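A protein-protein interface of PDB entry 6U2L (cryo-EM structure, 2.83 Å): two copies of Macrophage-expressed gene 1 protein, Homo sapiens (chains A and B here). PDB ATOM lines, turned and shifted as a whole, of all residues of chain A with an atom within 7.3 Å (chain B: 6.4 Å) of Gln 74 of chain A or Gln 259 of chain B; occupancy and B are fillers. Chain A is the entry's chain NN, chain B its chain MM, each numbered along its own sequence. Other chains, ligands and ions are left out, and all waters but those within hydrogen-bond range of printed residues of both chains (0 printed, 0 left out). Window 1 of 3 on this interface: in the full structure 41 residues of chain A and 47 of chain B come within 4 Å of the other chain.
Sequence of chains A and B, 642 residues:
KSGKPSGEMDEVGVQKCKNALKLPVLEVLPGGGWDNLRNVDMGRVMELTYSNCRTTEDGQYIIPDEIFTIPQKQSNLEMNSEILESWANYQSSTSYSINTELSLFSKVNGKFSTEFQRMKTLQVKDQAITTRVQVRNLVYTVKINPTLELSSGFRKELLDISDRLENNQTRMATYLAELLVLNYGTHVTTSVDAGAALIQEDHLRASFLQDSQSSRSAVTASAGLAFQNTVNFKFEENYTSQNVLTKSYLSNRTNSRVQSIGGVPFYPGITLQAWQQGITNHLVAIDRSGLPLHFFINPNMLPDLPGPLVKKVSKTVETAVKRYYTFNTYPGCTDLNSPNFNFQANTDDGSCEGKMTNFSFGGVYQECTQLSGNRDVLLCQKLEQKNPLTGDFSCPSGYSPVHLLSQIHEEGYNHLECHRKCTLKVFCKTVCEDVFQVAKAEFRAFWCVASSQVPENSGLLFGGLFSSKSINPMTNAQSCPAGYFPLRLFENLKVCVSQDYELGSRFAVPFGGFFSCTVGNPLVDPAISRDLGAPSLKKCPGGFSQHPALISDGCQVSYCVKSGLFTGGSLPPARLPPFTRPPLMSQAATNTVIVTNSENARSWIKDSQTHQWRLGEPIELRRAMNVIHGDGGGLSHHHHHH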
ATOM      1  N   PRO A  71      17.526 -12.038 -24.882  1.00  0.00           N
ATOM      2  CA  PRO A  71      16.737 -10.881 -24.451  1.00  0.00           C
ATOM      3  C   PRO A  71      15.327 -11.298 -24.074  1.00  0.00           C
ATOM      4  O   PRO A  71      14.523 -11.685 -24.926  1.00  0.00           O
ATOM      5  CB  PRO A  71      16.758  -9.970 -25.686  1.00  0.00           C
ATOM      6  CG  PRO A  71      16.965 -10.879 -26.811  1.00  0.00           C
ATOM      7  CD  PRO A  71      17.815 -11.995 -26.320  1.00  0.00           C
ATOM      8  N   GLN A  72      15.028 -11.251 -22.787  1.00  0.00           N
ATOM      9  CA  GLN A  72      13.661 -11.454 -22.335  1.00  0.00           C
ATOM     10  C   GLN A  72      13.350 -10.384 -21.305  1.00  0.00           C
ATOM     11  O   GLN A  72      13.481 -10.577 -20.101  1.00  0.00           O
ATOM     12  CB  GLN A  72      13.445 -12.882 -21.848  1.00  0.00           C
ATOM     13  CG  GLN A  72      14.435 -13.484 -20.894  1.00  0.00           C
ATOM     14  CD  GLN A  72      14.154 -14.945 -20.735  1.00  0.00           C
ATOM     15  OE1 GLN A  72      13.239 -15.475 -21.361  1.00  0.00           O
ATOM     16  NE2 GLN A  72      14.914 -15.608 -19.886  1.00  0.00           N
ATOM     17  N   LYS A  73      12.903  -9.241 -21.807  1.00  0.00           N
ATOM     18  CA  LYS A  73      12.774  -8.026 -21.021  1.00  0.00           C
ATOM     19  C   LYS A  73      11.428  -8.082 -20.315  1.00  0.00           C
ATOM     20  O   LYS A  73      10.426  -7.515 -20.745  1.00  0.00           O
ATOM     21  CB  LYS A  73      12.925  -6.817 -21.923  1.00  0.00           C
ATOM     22  CG  LYS A  73      14.286  -6.776 -22.537  1.00  0.00           C
ATOM     23  CD  LYS A  73      14.479  -5.601 -23.427  1.00  0.00           C
ATOM     24  CE  LYS A  73      15.877  -5.595 -23.979  1.00  0.00           C
ATOM     25  NZ  LYS A  73      16.090  -4.479 -24.914  1.00  0.00           N
ATOM     26  N   GLN A  74      11.424  -8.788 -19.198  1.00  0.00           N
ATOM     27  CA  GLN A  74      10.220  -9.269 -18.551  1.00  0.00           C
ATOM     28  C   GLN A  74      10.086  -8.639 -17.179  1.00  0.00           C
ATOM     29  O   GLN A  74      11.012  -8.697 -16.374  1.00  0.00           O
ATOM     30  CB  GLN A  74      10.275 -10.779 -18.440  1.00  0.00           C
ATOM     31  CG  GLN A  74       9.158 -11.404 -17.700  1.00  0.00           C
ATOM     32  CD  GLN A  74       9.344 -12.887 -17.607  1.00  0.00           C
ATOM     33  OE1 GLN A  74      10.260 -13.439 -18.201  1.00  0.00           O
ATOM     34  NE2 GLN A  74       8.523 -13.534 -16.811  1.00  0.00           N
ATOM     35  N   SER A  75       8.939  -8.041 -16.916  1.00  0.00           N
ATOM     36  CA  SER A  75       8.653  -7.397 -15.648  1.00  0.00           C
ATOM     37  C   SER A  75       7.457  -8.084 -15.014  1.00  0.00           C
ATOM     38  O   SER A  75       6.479  -8.376 -15.700  1.00  0.00           O
ATOM     39  CB  SER A  75       8.383  -5.913 -15.857  1.00  0.00           C
ATOM     40  OG  SER A  75       8.077  -5.275 -14.641  1.00  0.00           O
ATOM     41  N   ASN A  76       7.543  -8.371 -13.723  1.00  0.00           N
ATOM     42  CA  ASN A  76       6.469  -9.008 -12.976  1.00  0.00           C
ATOM     43  C   ASN A  76       6.085  -8.131 -11.805  1.00  0.00           C
ATOM     44  O   ASN A  76       6.949  -7.569 -11.136  1.00  0.00           O
ATOM     45  CB  ASN A  76       6.879 -10.369 -12.448  1.00  0.00           C
ATOM     46  CG  ASN A  76       7.108 -11.366 -13.536  1.00  0.00           C
ATOM     47  OD1 ASN A  76       8.237 -11.762 -13.801  1.00  0.00           O
ATOM     48  ND2 ASN A  76       6.034 -11.816 -14.150  1.00  0.00           N
ATOM     49  N   LEU A  77       4.792  -8.029 -11.542  1.00  0.00           N
ATOM     50  CA  LEU A  77       4.307  -7.199 -10.454  1.00  0.00           C
ATOM     51  C   LEU A  77       3.188  -7.953  -9.766  1.00  0.00           C
ATOM     52  O   LEU A  77       2.212  -8.335 -10.409  1.00  0.00           O
ATOM     53  CB  LEU A  77       3.814  -5.862 -10.987  1.00  0.00           C
ATOM     54  CG  LEU A  77       3.756  -4.642 -10.087  1.00  0.00           C
ATOM     55  CD1 LEU A  77       3.894  -3.475 -11.003  1.00  0.00           C
ATOM     56  CD2 LEU A  77       2.491  -4.527  -9.307  1.00  0.00           C
ATOM     57  N   GLU A  78       3.330  -8.178  -8.470  1.00  0.00           N
ATOM     58  CA  GLU A  78       2.328  -8.883  -7.689  1.00  0.00           C
ATOM     59  C   GLU A  78       1.483  -7.883  -6.923  1.00  0.00           C
ATOM     60  O   GLU A  78       2.020  -6.983  -6.277  1.00  0.00           O
ATOM     61  CB  GLU A  78       2.985  -9.855  -6.717  1.00  0.00           C
ATOM     62  CG  GLU A  78       3.661 -11.031  -7.359  1.00  0.00           C
ATOM     63  CD  GLU A  78       2.678 -12.007  -7.955  1.00  0.00           C
ATOM     64  OE1 GLU A  78       1.526 -12.070  -7.481  1.00  0.00           O
ATOM     65  OE2 GLU A  78       3.072 -12.750  -8.873  1.00  0.00           O
ATOM     66  N   ARG A 136       9.788  -8.178  -9.568  1.00  0.00           N
ATOM     67  CA  ARG A 136      10.959  -8.728 -10.225  1.00  0.00           C
ATOM     68  C   ARG A 136      11.039  -8.231 -11.654  1.00  0.00           C
ATOM     69  O   ARG A 136      10.026  -8.114 -12.337  1.00  0.00           O
ATOM     70  CB  ARG A 136      10.926 -10.246 -10.197  1.00  0.00           C
ATOM     71  CG  ARG A 136      11.027 -10.774  -8.811  1.00  0.00           C
ATOM     72  CD  ARG A 136      10.884 -12.261  -8.747  1.00  0.00           C
ATOM     73  NE  ARG A 136      11.979 -12.971  -9.384  1.00  0.00           N
ATOM     74  CZ  ARG A 136      13.113 -13.290  -8.777  1.00  0.00           C
ATOM     75  NH1 ARG A 136      14.039 -13.958  -9.432  1.00  0.00           N
ATOM     76  NH2 ARG A 136      13.323 -12.938  -7.521  1.00  0.00           N
ATOM     77  N   ASN A 137      12.250  -7.938 -12.104  1.00  0.00           N
ATOM     78  CA  ASN A 137      12.478  -7.313 -13.399  1.00  0.00           C
ATOM     79  C   ASN A 137      13.618  -8.061 -14.075  1.00  0.00           C
ATOM     80  O   ASN A 137      14.772  -7.668 -13.959  1.00  0.00           O
ATOM     81  CB  ASN A 137      12.769  -5.848 -13.193  1.00  0.00           C
ATOM     82  CG  ASN A 137      12.422  -5.004 -14.385  1.00  0.00           C
ATOM     83  OD1 ASN A 137      12.074  -3.840 -14.229  1.00  0.00           O
ATOM     84  ND2 ASN A 137      12.561  -5.556 -15.587  1.00  0.00           N
ATOM     85  N   LEU A 138      13.281  -9.122 -14.792  1.00  0.00           N
ATOM     86  CA  LEU A 138      14.243  -9.930 -15.527  1.00  0.00           C
ATOM     87  C   LEU A 138      14.548  -9.313 -16.883  1.00  0.00           C
ATOM     88  O   LEU A 138      13.641  -9.075 -17.672  1.00  0.00           O
ATOM     89  CB  LEU A 138      13.680 -11.332 -15.699  1.00  0.00           C
ATOM     90  CG  LEU A 138      14.395 -12.311 -16.609  1.00  0.00           C
ATOM     91  CD1 LEU A 138      15.792 -12.476 -16.194  1.00  0.00           C
ATOM     92  CD2 LEU A 138      13.697 -13.645 -16.535  1.00  0.00           C
ATOM     93  N   VAL A 139      15.819  -9.072 -17.167  1.00  0.00           N
ATOM     94  CA  VAL A 139      16.232  -8.395 -18.387  1.00  0.00           C
ATOM     95  C   VAL A 139      16.907  -9.354 -19.362  1.00  0.00           C
ATOM     96  O   VAL A 139      16.528  -9.426 -20.527  1.00  0.00           O
ATOM     97  CB  VAL A 139      17.142  -7.190 -18.073  1.00  0.00           C
ATOM     98  CG1 VAL A 139      17.477  -6.455 -19.335  1.00  0.00           C
ATOM     99  CG2 VAL A 139      16.475  -6.273 -17.094  1.00  0.00           C
ATOM    100  N   TYR A 140      17.909 -10.101 -18.906  1.00  0.00           N
ATOM    101  CA  TYR A 140      18.619 -11.037 -19.764  1.00  0.00           C
ATOM    102  C   TYR A 140      18.698 -12.411 -19.128  1.00  0.00           C
ATOM    103  O   TYR A 140      18.675 -12.551 -17.908  1.00  0.00           O
ATOM    104  CB  TYR A 140      20.047 -10.594 -20.062  1.00  0.00           C
ATOM    105  CG  TYR A 140      20.154  -9.349 -20.877  1.00  0.00           C
ATOM    106  CD1 TYR A 140      19.892  -9.366 -22.233  1.00  0.00           C
ATOM    107  CD2 TYR A 140      20.546  -8.161 -20.297  1.00  0.00           C
ATOM    108  CE1 TYR A 140      19.990  -8.233 -22.976  1.00  0.00           C
ATOM    109  CE2 TYR A 140      20.643  -7.024 -21.031  1.00  0.00           C
ATOM    110  CZ  TYR A 140      20.365  -7.064 -22.367  1.00  0.00           C
ATOM    111  OH  TYR A 140      20.469  -5.916 -23.103  1.00  0.00           O
ATOM    112  N   ALA A 196      16.796  -7.045 -11.657  1.00  0.00           N
ATOM    113  CA  ALA A 196      16.652  -6.425 -10.353  1.00  0.00           C
ATOM    114  C   ALA A 196      15.383  -6.929  -9.690  1.00  0.00           C
ATOM    115  O   ALA A 196      14.492  -7.457 -10.343  1.00  0.00           O
ATOM    116  CB  ALA A 196      16.619  -4.909 -10.465  1.00  0.00           C
ATOM    117  N   ILE A 286      19.526 -12.446 -10.290  1.00  0.00           N
ATOM    118  CA  ILE A 286      18.347 -12.738  -9.492  1.00  0.00           C
ATOM    119  C   ILE A 286      17.926 -14.192  -9.592  1.00  0.00           C
ATOM    120  O   ILE A 286      17.014 -14.605  -8.865  1.00  0.00           O
ATOM    121  CB  ILE A 286      17.168 -11.815  -9.861  1.00  0.00           C
ATOM    122  CG1 ILE A 286      16.804 -11.960 -11.332  1.00  0.00           C
ATOM    123  CG2 ILE A 286      17.498 -10.387  -9.522  1.00  0.00           C
ATOM    124  CD1 ILE A 286      15.575 -11.232 -11.698  1.00  0.00           C
ATOM    125  N   SER B  93       1.008 -18.634 -23.694  1.00  0.00           N
ATOM    126  CA  SER B  93       1.016 -17.179 -23.913  1.00  0.00           C
ATOM    127  C   SER B  93       2.343 -16.613 -24.398  1.00  0.00           C
ATOM    128  O   SER B  93       2.413 -15.421 -24.683  1.00  0.00           O
ATOM    129  CB  SER B  93       0.610 -16.362 -22.679  1.00  0.00           C
ATOM    130  OG  SER B  93       1.635 -16.390 -21.708  1.00  0.00           O
ATOM    131  N   GLU B 115       6.098 -20.891 -15.781  1.00  0.00           N
ATOM    132  CA  GLU B 115       4.809 -20.249 -15.957  1.00  0.00           C
ATOM    133  C   GLU B 115       3.663 -21.235 -15.786  1.00  0.00           C
ATOM    134  O   GLU B 115       2.577 -20.847 -15.351  1.00  0.00           O
ATOM    135  CB  GLU B 115       4.777 -19.582 -17.333  1.00  0.00           C
ATOM    136  CG  GLU B 115       3.581 -18.707 -17.623  1.00  0.00           C
ATOM    137  CD  GLU B 115       3.530 -17.459 -16.770  1.00  0.00           C
ATOM    138  OE1 GLU B 115       4.597 -16.957 -16.364  1.00  0.00           O
ATOM    139  OE2 GLU B 115       2.407 -16.982 -16.498  1.00  0.00           O
ATOM    140  N   ALA B 197       4.223  -7.694 -25.053  1.00  0.00           N
ATOM    141  CA  ALA B 197       2.917  -8.048 -24.526  1.00  0.00           C
ATOM    142  C   ALA B 197       2.817  -7.577 -23.088  1.00  0.00           C
ATOM    143  O   ALA B 197       3.803  -7.568 -22.359  1.00  0.00           O
ATOM    144  CB  ALA B 197       2.659  -9.549 -24.602  1.00  0.00           C
ATOM    145  N   LEU B 198       1.615  -7.194 -22.683  1.00  0.00           N
ATOM    146  CA  LEU B 198       1.343  -6.793 -21.311  1.00  0.00           C
ATOM    147  C   LEU B 198       0.203  -7.670 -20.828  1.00  0.00           C
ATOM    148  O   LEU B 198      -0.892  -7.593 -21.373  1.00  0.00           O
ATOM    149  CB  LEU B 198       0.951  -5.318 -21.243  1.00  0.00           C
ATOM    150  CG  LEU B 198       1.246  -4.492 -19.990  1.00  0.00           C
ATOM    151  CD1 LEU B 198       1.041  -3.034 -20.297  1.00  0.00           C
ATOM    152  CD2 LEU B 198       0.458  -4.887 -18.752  1.00  0.00           C
ATOM    153  N   ILE B 199       0.438  -8.483 -19.806  1.00  0.00           N
ATOM    154  CA  ILE B 199      -0.479  -9.554 -19.433  1.00  0.00           C
ATOM    155  C   ILE B 199      -0.953  -9.353 -17.997  1.00  0.00           C
ATOM    156  O   ILE B 199      -0.153  -9.051 -17.108  1.00  0.00           O
ATOM    157  CB  ILE B 199       0.192 -10.928 -19.605  1.00  0.00           C
ATOM    158  CG1 ILE B 199       0.631 -11.120 -21.051  1.00  0.00           C
ATOM    159  CG2 ILE B 199      -0.739 -12.051 -19.250  1.00  0.00           C
ATOM    160  CD1 ILE B 199       1.470 -12.319 -21.263  1.00  0.00           C
ATOM    161  N   GLN B 200      -2.255  -9.512 -17.782  1.00  0.00           N
ATOM    162  CA  GLN B 200      -2.893  -9.611 -16.476  1.00  0.00           C
ATOM    163  C   GLN B 200      -3.248 -11.060 -16.207  1.00  0.00           C
ATOM    164  O   GLN B 200      -3.743 -11.746 -17.092  1.00  0.00           O
ATOM    165  CB  GLN B 200      -4.171  -8.785 -16.467  1.00  0.00           C
ATOM    166  CG  GLN B 200      -5.019  -8.823 -15.221  1.00  0.00           C
ATOM    167  CD  GLN B 200      -4.487  -7.978 -14.129  1.00  0.00           C
ATOM    168  OE1 GLN B 200      -4.028  -6.875 -14.366  1.00  0.00           O
ATOM    169  NE2 GLN B 200      -4.570  -8.472 -12.910  1.00  0.00           N
ATOM    170  N   GLU B 201      -3.035 -11.527 -14.989  1.00  0.00           N
ATOM    171  CA  GLU B 201      -3.404 -12.901 -14.663  1.00  0.00           C
ATOM    172  C   GLU B 201      -3.987 -12.928 -13.256  1.00  0.00           C
ATOM    173  O   GLU B 201      -3.243 -12.928 -12.275  1.00  0.00           O
ATOM    174  CB  GLU B 201      -2.210 -13.827 -14.781  1.00  0.00           C
ATOM    175  CG  GLU B 201      -2.557 -15.287 -14.616  1.00  0.00           C
ATOM    176  CD  GLU B 201      -1.331 -16.175 -14.670  1.00  0.00           C
ATOM    177  OE1 GLU B 201      -0.210 -15.628 -14.754  1.00  0.00           O
ATOM    178  OE2 GLU B 201      -1.480 -17.414 -14.632  1.00  0.00           O
ATOM    179  N   ARG B 257      -1.448 -11.318 -10.551  1.00  0.00           N
ATOM    180  CA  ARG B 257      -0.161 -10.847 -11.061  1.00  0.00           C
ATOM    181  C   ARG B 257      -0.337  -9.995 -12.317  1.00  0.00           C
ATOM    182  O   ARG B 257      -1.248 -10.215 -13.110  1.00  0.00           O
ATOM    183  CB  ARG B 257       0.734 -12.038 -11.387  1.00  0.00           C
ATOM    184  CG  ARG B 257       2.176 -11.722 -11.638  1.00  0.00           C
ATOM    185  CD  ARG B 257       2.934 -12.949 -12.053  1.00  0.00           C
ATOM    186  NE  ARG B 257       2.443 -13.435 -13.333  1.00  0.00           N
ATOM    187  CZ  ARG B 257       2.853 -14.553 -13.907  1.00  0.00           C
ATOM    188  NH1 ARG B 257       2.348 -14.925 -15.071  1.00  0.00           N
ATOM    189  NH2 ARG B 257       3.778 -15.292 -13.319  1.00  0.00           N
ATOM    190  N   VAL B 258       0.549  -9.020 -12.499  1.00  0.00           N
ATOM    191  CA  VAL B 258       0.642  -8.252 -13.738  1.00  0.00           C
ATOM    192  C   VAL B 258       2.032  -8.449 -14.320  1.00  0.00           C
ATOM    193  O   VAL B 258       3.029  -8.207 -13.637  1.00  0.00           O
ATOM    194  CB  VAL B 258       0.366  -6.757 -13.512  1.00  0.00           C
ATOM    195  CG1 VAL B 258       0.520  -6.026 -14.786  1.00  0.00           C
ATOM    196  CG2 VAL B 258      -1.015  -6.554 -13.003  1.00  0.00           C
ATOM    197  N   GLN B 259       2.101  -8.870 -15.577  1.00  0.00           N
ATOM    198  CA  GLN B 259       3.362  -9.245 -16.197  1.00  0.00           C
ATOM    199  C   GLN B 259       3.574  -8.473 -17.484  1.00  0.00           C
ATOM    200  O   GLN B 259       2.688  -8.427 -18.335  1.00  0.00           O
ATOM    201  CB  GLN B 259       3.392 -10.729 -16.497  1.00  0.00           C
ATOM    202  CG  GLN B 259       4.708 -11.206 -16.995  1.00  0.00           C
ATOM    203  CD  GLN B 259       4.675 -12.651 -17.383  1.00  0.00           C
ATOM    204  OE1 GLN B 259       3.618 -13.269 -17.412  1.00  0.00           O
ATOM    205  NE2 GLN B 259       5.832 -13.212 -17.665  1.00  0.00           N
ATOM    206  N   SER B 260       4.750  -7.886 -17.635  1.00  0.00           N
ATOM    207  CA  SER B 260       5.160  -7.240 -18.872  1.00  0.00           C
ATOM    208  C   SER B 260       6.231  -8.091 -19.533  1.00  0.00           C
ATOM    209  O   SER B 260       7.173  -8.519 -18.875  1.00  0.00           O
ATOM    210  CB  SER B 260       5.690  -5.840 -18.594  1.00  0.00           C
ATOM    211  OG  SER B 260       6.148  -5.228 -19.773  1.00  0.00           O
ATOM    212  N   ILE B 261       6.074  -8.360 -20.818  1.00  0.00           N
ATOM    213  CA  ILE B 261       7.035  -9.149 -21.578  1.00  0.00           C
ATOM    214  C   ILE B 261       7.490  -8.292 -22.747  1.00  0.00           C
ATOM    215  O   ILE B 261       6.745  -8.106 -23.710  1.00  0.00           O
ATOM    216  CB  ILE B 261       6.442 -10.473 -22.065  1.00  0.00           C
ATOM    217  CG1 ILE B 261       6.018 -11.332 -20.887  1.00  0.00           C
ATOM    218  CG2 ILE B 261       7.439 -11.230 -22.850  1.00  0.00           C
ATOM    219  CD1 ILE B 261       5.236 -12.532 -21.287  1.00  0.00           C
ATOM    220  N   GLY B 262       8.700  -7.769 -22.669  1.00  0.00           N
ATOM    221  CA  GLY B 262       9.193  -6.858 -23.674  1.00  0.00           C
ATOM    222  C   GLY B 262       8.752  -5.437 -23.406  1.00  0.00           C
ATOM    223  O   GLY B 262       7.905  -5.159 -22.560  1.00  0.00           O
ATOM    224  N   PHE B 266       6.743  -2.373 -16.639  1.00  0.00           N
ATOM    225  CA  PHE B 266       5.437  -1.899 -16.233  1.00  0.00           C
ATOM    226  C   PHE B 266       5.474  -1.354 -14.815  1.00  0.00           C
ATOM    227  O   PHE B 266       6.166  -1.883 -13.943  1.00  0.00           O
ATOM    228  CB  PHE B 266       4.411  -3.025 -16.328  1.00  0.00           C
ATOM    229  CG  PHE B 266       3.037  -2.616 -15.918  1.00  0.00           C
ATOM    230  CD1 PHE B 266       2.268  -1.833 -16.746  1.00  0.00           C
ATOM    231  CD2 PHE B 266       2.519  -2.997 -14.694  1.00  0.00           C
ATOM    232  CE1 PHE B 266       1.010  -1.445 -16.369  1.00  0.00           C
ATOM    233  CE2 PHE B 266       1.262  -2.601 -14.313  1.00  0.00           C
ATOM    234  CZ  PHE B 266       0.507  -1.833 -15.155  1.00  0.00           C
ATOM    235  N   VAL B 284      10.953  -8.863 -27.853  1.00  0.00           N
ATOM    236  CA  VAL B 284      11.241 -10.214 -27.410  1.00  0.00           C
ATOM    237  C   VAL B 284      10.410 -11.167 -28.247  1.00  0.00           C
ATOM    238  O   VAL B 284       9.562 -10.758 -29.031  1.00  0.00           O
ATOM    239  CB  VAL B 284      10.951 -10.422 -25.912  1.00  0.00           C
ATOM    240  CG1 VAL B 284      11.852  -9.563 -25.067  1.00  0.00           C
ATOM    241  CG2 VAL B 284       9.536 -10.090 -25.637  1.00  0.00           C
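The backbone carbonyl oxygen (O) of Val 258 of chain B sits at hydrogen-bond distance from the backbone NH (N) of Leu 77 of chain A (2.7 Å). The side-chain amide nitrogen (NE2) of Gln 259 of chain B sits close to the side-chain amide nitrogen (NE2) of Gln 74 of chain A (2.8 Å). The backbone NH (N) of Ser 260 of chain B sits at hydrogen-bond distance from the backbone carbonyl oxygen (O) of Ser 75 of chain A. N of Gly 262 of chain B sits at hydrogen-bond distance from O of Lys 73 of chain A (2.6 Å).
The side-chain hydroxyl of Ser 260 of chain B sits at hydrogen-bond distance from the backbone carbonyl oxygen of Gly 262 of chain B (3.3 Å). O of Leu 138 of chain A is in hydrogen-bond range of N of Gln 74 of chain A (2.7 Å). The backbone NH of Ile 261 of chain B lies within hydrogen-bond range of the backbone carbonyl oxygen of Ala 197 of chain B, at 2.9 Å. The guanidinium group of Arg 257 of chain B is in salt-bridge range of the side-chain carboxylate of Glu 115 of chain B (2.5 Å). O of Arg 136 of chain A sits at hydrogen-bond distance from N of Asn 76 of chain A (2.9 Å). The backbone NH (N) of Ile 199 of chain B lies within hydrogen-bond range of the backbone carbonyl oxygen (O) of Gln 259 of chain B, at 2.7 Å.
Pro 71 of chain A touches Val 284 of chain B. CA of Gln 72 of chain A touches CG1 of Val 284 of chain B (3.8 Å). Ser 260 of chain B touches Lys 73 of chain A. Lys 73 of chain A touches Val 284 of chain B (N to CG1, 3.4 Å). O of Ser 260 of chain B touches CA of Gln 74 of chain A (3.2 Å). Ser 75 of chain A touches Gln 259 of chain B (O to CA, 3.3 Å). C of Asn 76 of chain A touches O of Val 258 of chain B, 3.6 Å away. Arg 257 of chain B touches Leu 77 of chain A. CD1 of Leu 77 of chain A touches CD2 of Phe 266 of chain B, 3.97 Å away. Glu 78 of chain A touches Arg 257 of chain B.
Printed residues of chain B within 4 Å of Pro 71 of chain A: Val 284 (3.4 Å). Of the printed residues of chain B, Gln 72 of chain A touches Val 284 (3.8 Å). Of chain B, only Gln 259 and Ser 260 come within 4 Å of Gln 74 of chain A. Ala 197 of chain B touches none of the printed residues of chain A. Printed residues of chain A within 4 Å of Arg 257 of chain B: Asn 76, Leu 77 and Glu 78. Of chain A, only Gln 74 (2.8 Å), Ser 75 (3.3 Å) and Asn 76 (3.2 Å) come within 4 Å of Gln 259 of chain B. Of the printed residues of chain A, Ser 260 of chain B touches Lys 73 (3.9 Å), Gln 74 (3.2 Å) and Ser 75 (2.6 Å). The nearest residue of chain A that does not touch Gln 259 of chain B is Leu 77 of chain A (4.9 Å).
Of the 15 printed residues of chain A, 8 touch a printed residue of chain B.
No position is printed for both chains. Of the 18 pairs that touch across the chains among the printed residues, none has its exchanged pair printed and touching as well.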
